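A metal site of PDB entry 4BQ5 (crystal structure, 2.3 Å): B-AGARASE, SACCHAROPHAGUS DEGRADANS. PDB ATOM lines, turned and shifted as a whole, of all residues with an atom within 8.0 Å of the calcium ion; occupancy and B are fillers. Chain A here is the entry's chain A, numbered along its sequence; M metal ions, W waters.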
ATOM      1  N   MET A   4      17.110 -27.451  -9.155  1.00  0.00           N
ATOM      2  CA  MET A   4      18.038 -26.366  -9.412  1.00  0.00           C
ATOM      3  C   MET A   4      19.388 -26.516  -8.690  1.00  0.00           C
ATOM      4  O   MET A   4      19.450 -26.756  -7.471  1.00  0.00           O
ATOM      5  CB  MET A   4      17.398 -25.030  -9.034  1.00  0.00           C
ATOM      6  CG  MET A   4      18.287 -23.809  -9.305  1.00  0.00           C
ATOM      7  SD  MET A   4      18.520 -23.429 -11.064  1.00  0.00           S
ATOM      8  CE  MET A   4      16.830 -23.151 -11.647  1.00  0.00           C
ATOM      9  N   PHE A   6      22.394 -24.368  -9.952  1.00  0.00           N
ATOM     10  CA  PHE A   6      23.048 -23.038 -10.029  1.00  0.00           C
ATOM     11  C   PHE A   6      22.203 -22.035 -10.812  1.00  0.00           C
ATOM     12  O   PHE A   6      22.141 -22.085 -12.063  1.00  0.00           O
ATOM     13  CB  PHE A   6      24.464 -23.080 -10.689  1.00  0.00           C
ATOM     14  CG  PHE A   6      25.480 -23.953  -9.970  1.00  0.00           C
ATOM     15  CD1 PHE A   6      26.205 -23.463  -8.894  1.00  0.00           C
ATOM     16  CD2 PHE A   6      25.704 -25.258 -10.385  1.00  0.00           C
ATOM     17  CE1 PHE A   6      27.131 -24.260  -8.239  1.00  0.00           C
ATOM     18  CE2 PHE A   6      26.636 -26.061  -9.751  1.00  0.00           C
ATOM     19  CZ  PHE A   6      27.344 -25.579  -8.668  1.00  0.00           C
ATOM     20  N   ASP A   7      21.593 -21.110 -10.066  1.00  0.00           N
ATOM     21  CA  ASP A   7      20.860 -19.981 -10.694  1.00  0.00           C
ATOM     22  C   ASP A   7      21.564 -18.632 -10.523  1.00  0.00           C
ATOM     23  O   ASP A   7      21.138 -17.617 -11.074  1.00  0.00           O
ATOM     24  CB  ASP A   7      19.417 -19.901 -10.191  1.00  0.00           C
ATOM     25  CG  ASP A   7      19.309 -19.542  -8.697  1.00  0.00           C
ATOM     26  OD1 ASP A   7      20.261 -18.957  -8.068  1.00  0.00           O
ATOM     27  OD2 ASP A   7      18.215 -19.845  -8.166  1.00  0.00           O
ATOM     28  N   PHE A   8      22.631 -18.634  -9.728  1.00  0.00           N
ATOM     29  CA  PHE A   8      23.477 -17.475  -9.562  1.00  0.00           C
ATOM     30  C   PHE A   8      22.747 -16.240  -9.009  1.00  0.00           C
ATOM     31  O   PHE A   8      23.217 -15.121  -9.147  1.00  0.00           O
ATOM     32  CB  PHE A   8      24.227 -17.138 -10.874  1.00  0.00           C
ATOM     33  CG  PHE A   8      24.958 -18.311 -11.462  1.00  0.00           C
ATOM     34  CD1 PHE A   8      26.096 -18.813 -10.833  1.00  0.00           C
ATOM     35  CD2 PHE A   8      24.498 -18.933 -12.606  1.00  0.00           C
ATOM     36  CE1 PHE A   8      26.763 -19.921 -11.356  1.00  0.00           C
ATOM     37  CE2 PHE A   8      25.158 -20.039 -13.141  1.00  0.00           C
ATOM     38  CZ  PHE A   8      26.292 -20.528 -12.507  1.00  0.00           C
ATOM     39  N   GLU A   9      21.605 -16.444  -8.364  1.00  0.00           N
ATOM     40  CA  GLU A   9      20.817 -15.292  -7.930  1.00  0.00           C
ATOM     41  C   GLU A   9      21.362 -14.712  -6.612  1.00  0.00           C
ATOM     42  O   GLU A   9      21.020 -13.584  -6.230  1.00  0.00           O
ATOM     43  CB  GLU A   9      19.322 -15.645  -7.857  1.00  0.00           C
ATOM     44  CG  GLU A   9      18.641 -15.692  -9.203  1.00  0.00           C
ATOM     45  CD  GLU A   9      18.882 -14.457 -10.036  1.00  0.00           C
ATOM     46  OE1 GLU A   9      18.656 -13.332  -9.530  1.00  0.00           O
ATOM     47  OE2 GLU A   9      19.299 -14.604 -11.209  1.00  0.00           O
ATOM     48  N   ASN A  10      22.205 -15.488  -5.958  1.00  0.00           N
ATOM     49  CA  ASN A  10      22.969 -15.022  -4.793  1.00  0.00           C
ATOM     50  C   ASN A  10      24.186 -14.174  -5.211  1.00  0.00           C
ATOM     51  O   ASN A  10      24.946 -13.747  -4.349  1.00  0.00           O
ATOM     52  CB  ASN A  10      23.394 -16.220  -3.905  1.00  0.00           C
ATOM     53  CG  ASN A  10      24.384 -17.173  -4.610  1.00  0.00           C
ATOM     54  OD1 ASN A  10      24.953 -16.861  -5.673  1.00  0.00           O
ATOM     55  ND2 ASN A  10      24.597 -18.337  -4.001  1.00  0.00           N
ATOM     56  N   ILE A  26      29.743 -12.389 -12.410  1.00  0.00           N
ATOM     57  CA  ILE A  26      28.291 -12.451 -12.451  1.00  0.00           C
ATOM     58  C   ILE A  26      27.816 -11.139 -13.048  1.00  0.00           C
ATOM     59  O   ILE A  26      28.421 -10.098 -12.826  1.00  0.00           O
ATOM     60  CB  ILE A  26      27.619 -12.741 -11.073  1.00  0.00           C
ATOM     61  CG1 ILE A  26      28.285 -13.904 -10.334  1.00  0.00           C
ATOM     62  CG2 ILE A  26      26.136 -13.068 -11.271  1.00  0.00           C
ATOM     63  CD1 ILE A  26      28.190 -15.261 -11.020  1.00  0.00           C
ATOM     64  N   GLU A  27      26.755 -11.227 -13.851  1.00  0.00           N
ATOM     65  CA  GLU A  27      26.247 -10.103 -14.602  1.00  0.00           C
ATOM     66  C   GLU A  27      24.760 -10.272 -14.681  1.00  0.00           C
ATOM     67  O   GLU A  27      24.231 -11.392 -14.626  1.00  0.00           O
ATOM     68  CB  GLU A  27      26.783 -10.120 -16.041  1.00  0.00           C
ATOM     69  CG  GLU A  27      28.163  -9.498 -16.263  1.00  0.00           C
ATOM     70  CD  GLU A  27      28.381  -9.010 -17.711  1.00  0.00           C
ATOM     71  OE1 GLU A  27      27.417  -9.033 -18.519  1.00  0.00           O
ATOM     72  OE2 GLU A  27      29.517  -8.603 -18.052  1.00  0.00           O
ATOM     73  N   TYR A  29      21.605 -10.225 -17.109  1.00  0.00           N
ATOM     74  CA  TYR A  29      21.299 -10.404 -18.517  1.00  0.00           C
ATOM     75  C   TYR A  29      19.779 -10.647 -18.677  1.00  0.00           C
ATOM     76  O   TYR A  29      19.058 -10.806 -17.702  1.00  0.00           O
ATOM     77  CB  TYR A  29      22.166 -11.557 -19.102  1.00  0.00           C
ATOM     78  CG  TYR A  29      21.591 -12.895 -18.742  1.00  0.00           C
ATOM     79  CD1 TYR A  29      21.734 -13.419 -17.443  1.00  0.00           C
ATOM     80  CD2 TYR A  29      20.842 -13.597 -19.647  1.00  0.00           C
ATOM     81  CE1 TYR A  29      21.134 -14.625 -17.096  1.00  0.00           C
ATOM     82  CE2 TYR A  29      20.257 -14.798 -19.317  1.00  0.00           C
ATOM     83  CZ  TYR A  29      20.396 -15.313 -18.046  1.00  0.00           C
ATOM     84  OH  TYR A  29      19.780 -16.523 -17.741  1.00  0.00           O
ATOM     85  N   GLY A  31      16.957 -13.046 -19.411  1.00  0.00           N
ATOM     86  CA  GLY A  31      16.752 -14.500 -19.411  1.00  0.00           C
ATOM     87  C   GLY A  31      15.857 -15.027 -20.533  1.00  0.00           C
ATOM     88  O   GLY A  31      15.169 -14.241 -21.205  1.00  0.00           O
ATOM     89  N   PRO A  36      15.191  -9.847 -16.588  1.00  0.00           N
ATOM     90  CA  PRO A  36      16.555  -9.737 -16.086  1.00  0.00           C
ATOM     91  C   PRO A  36      16.878 -10.794 -15.020  1.00  0.00           C
ATOM     92  O   PRO A  36      16.202 -10.863 -13.976  1.00  0.00           O
ATOM     93  CB  PRO A  36      16.596  -8.338 -15.450  1.00  0.00           C
ATOM     94  CG  PRO A  36      15.180  -7.852 -15.438  1.00  0.00           C
ATOM     95  CD  PRO A  36      14.537  -8.534 -16.602  1.00  0.00           C
ATOM     96  N   SER A  37      17.912 -11.577 -15.260  1.00  0.00           N
ATOM     97  CA  SER A  37      18.393 -12.552 -14.288  1.00  0.00           C
ATOM     98  C   SER A  37      19.910 -12.351 -14.046  1.00  0.00           C
ATOM     99  O   SER A  37      20.595 -11.731 -14.848  1.00  0.00           O
ATOM    100  CB  SER A  37      18.103 -13.960 -14.846  1.00  0.00           C
ATOM    101  OG  SER A  37      18.355 -14.978 -13.897  1.00  0.00           O
ATOM    102  N   LYS A  38      20.418 -12.844 -12.923  1.00  0.00           N
ATOM    103  CA  LYS A  38      21.849 -13.015 -12.758  1.00  0.00           C
ATOM    104  C   LYS A  38      22.397 -14.245 -13.530  1.00  0.00           C
ATOM    105  O   LYS A  38      21.792 -15.347 -13.544  1.00  0.00           O
ATOM    106  CB  LYS A  38      22.212 -13.132 -11.283  1.00  0.00           C
ATOM    107  CG  LYS A  38      21.970 -11.877 -10.442  1.00  0.00           C
ATOM    108  CD  LYS A  38      22.694 -10.638 -10.988  1.00  0.00           C
ATOM    109  CE  LYS A  38      22.777  -9.544  -9.918  1.00  0.00           C
ATOM    110  NZ  LYS A  38      21.701  -9.752  -8.875  1.00  0.00           N
ATOM    111  N   GLY A  39      23.557 -14.059 -14.155  1.00  0.00           N
ATOM    112  CA  GLY A  39      24.168 -15.154 -14.874  1.00  0.00           C
ATOM    113  C   GLY A  39      25.653 -15.224 -14.659  1.00  0.00           C
ATOM    114  O   GLY A  39      26.268 -14.236 -14.257  1.00  0.00           O
ATOM    115  N   LEU A  40      26.226 -16.394 -14.947  1.00  0.00           N
ATOM    116  CA  LEU A  40      27.693 -16.562 -14.998  1.00  0.00           C
ATOM    117  C   LEU A  40      28.210 -16.307 -16.415  1.00  0.00           C
ATOM    118  O   LEU A  40      27.962 -17.102 -17.352  1.00  0.00           O
ATOM    119  CB  LEU A  40      28.136 -17.941 -14.497  1.00  0.00           C
ATOM    120  CG  LEU A  40      29.658 -18.178 -14.529  1.00  0.00           C
ATOM    121  CD1 LEU A  40      30.311 -17.720 -13.215  1.00  0.00           C
ATOM    122  CD2 LEU A  40      29.936 -19.652 -14.797  1.00  0.00           C
ATOM    123  N   ASP A  75      21.081 -23.133 -19.421  1.00  0.00           N
ATOM    124  CA  ASP A  75      20.838 -21.964 -20.284  1.00  0.00           C
ATOM    125  C   ASP A  75      22.151 -21.343 -20.715  1.00  0.00           C
ATOM    126  O   ASP A  75      22.999 -21.032 -19.869  1.00  0.00           O
ATOM    127  CB  ASP A  75      20.019 -20.914 -19.543  1.00  0.00           C
ATOM    128  CG  ASP A  75      18.622 -21.370 -19.251  1.00  0.00           C
ATOM    129  OD1 ASP A  75      18.327 -22.541 -19.573  1.00  0.00           O
ATOM    130  OD2 ASP A  75      17.828 -20.564 -18.735  1.00  0.00           O
ATOM    131  N   ILE A 184      26.096 -18.325 -18.864  1.00  0.00           N
ATOM    132  CA  ILE A 184      25.457 -19.544 -18.376  1.00  0.00           C
ATOM    133  C   ILE A 184      24.545 -19.219 -17.196  1.00  0.00           C
ATOM    134  O   ILE A 184      24.908 -18.424 -16.322  1.00  0.00           O
ATOM    135  CB  ILE A 184      26.526 -20.579 -17.943  1.00  0.00           C
ATOM    136  CG1 ILE A 184      27.504 -20.784 -19.108  1.00  0.00           C
ATOM    137  CG2 ILE A 184      25.865 -21.910 -17.551  1.00  0.00           C
ATOM    138  CD1 ILE A 184      28.817 -21.429 -18.713  1.00  0.00           C
ATOM    139  N   ASP A 185      23.371 -19.857 -17.182  1.00  0.00           N
ATOM    140  CA  ASP A 185      22.392 -19.740 -16.094  1.00  0.00           C
ATOM    141  C   ASP A 185      21.492 -20.973 -15.944  1.00  0.00           C
ATOM    142  O   ASP A 185      21.273 -21.743 -16.899  1.00  0.00           O
ATOM    143  CB  ASP A 185      21.530 -18.464 -16.266  1.00  0.00           C
ATOM    144  CG  ASP A 185      20.810 -18.017 -14.975  1.00  0.00           C
ATOM    145  OD1 ASP A 185      21.088 -18.523 -13.869  1.00  0.00           O
ATOM    146  OD2 ASP A 185      19.939 -17.127 -15.064  1.00  0.00           O
ATOM    147  N   ASN A 186      21.014 -21.156 -14.713  1.00  0.00           N
ATOM    148  CA  ASN A 186      19.948 -22.098 -14.390  1.00  0.00           C
ATOM    149  C   ASN A 186      20.384 -23.521 -14.675  1.00  0.00           C
ATOM    150  O   ASN A 186      19.685 -24.291 -15.352  1.00  0.00           O
ATOM    151  CB  ASN A 186      18.633 -21.748 -15.103  1.00  0.00           C
ATOM    152  CG  ASN A 186      18.099 -20.369 -14.708  1.00  0.00           C
ATOM    153  OD1 ASN A 186      18.148 -19.962 -13.543  1.00  0.00           O
ATOM    154  ND2 ASN A 186      17.568 -19.649 -15.702  1.00  0.00           N
ATOM    155  N   ILE A 187      21.554 -23.867 -14.152  1.00  0.00           N
ATOM    156  CA  ILE A 187      22.050 -25.225 -14.251  1.00  0.00           C
ATOM    157  C   ILE A 187      21.125 -26.023 -13.324  1.00  0.00           C
ATOM    158  O   ILE A 187      21.018 -25.715 -12.137  1.00  0.00           O
ATOM    159  CB  ILE A 187      23.532 -25.342 -13.823  1.00  0.00           C
ATOM    160  CG1 ILE A 187      24.382 -24.238 -14.485  1.00  0.00           C
ATOM    161  CG2 ILE A 187      24.084 -26.740 -14.117  1.00  0.00           C
ATOM    162  CD1 ILE A 187      25.838 -24.227 -14.079  1.00  0.00           C
HETATM  163 CA    CA M   1      19.980 -16.567 -12.743  1.00  0.00          CA
HETATM  164  O   HOH W   1      17.791 -17.736 -12.752  1.00  0.00           O
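The side-chain hydroxyl of Tyr 29 sits close to the side-chain carboxylate of Asp 185, 2.7 Å away. The backbone carbonyl oxygen of Asp 185 lies within hydrogen-bond range of the backbone NH of Asp 75. O of Tyr 29 sits at hydrogen-bond distance from N of Ser 37, at 2.8 Å. ND2 of Asn 186 sits at hydrogen-bond distance from OD2 of Asp 75, 3.2 Å away. The backbone NH (N) of Asn 186 sits at hydrogen-bond distance from the backbone carbonyl oxygen (O) of Phe 6 (3.0 Å). The side-chain carboxylate (OD1) of Asp 185 lies close to the side-chain amide oxygen (OD1) of Asn 186 (3.3 Å).
Asn 186 touches the calcium ion (OD1 to CA, 3.9 Å). The nearest printed residue that does not touch the calcium ion is Phe 8 (4.5 Å).
The calcium ion is bound by the backbone carbonyl oxygen (O) of Asp 7 (2.3 Å), the backbone carbonyl oxygen (O) of Lys 38 (2.3 Å), the side-chain carboxylate (OD2) of Asp 185 (2.4 Å), water W1 (2.5 Å), the side-chain carboxylate (OD1) of Asp 185 (2.5 Å), the side-chain hydroxyl (OG) of Ser 37 (2.5 Å) and the side-chain carboxylate (OE2) of Glu 9 (2.6 Å).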
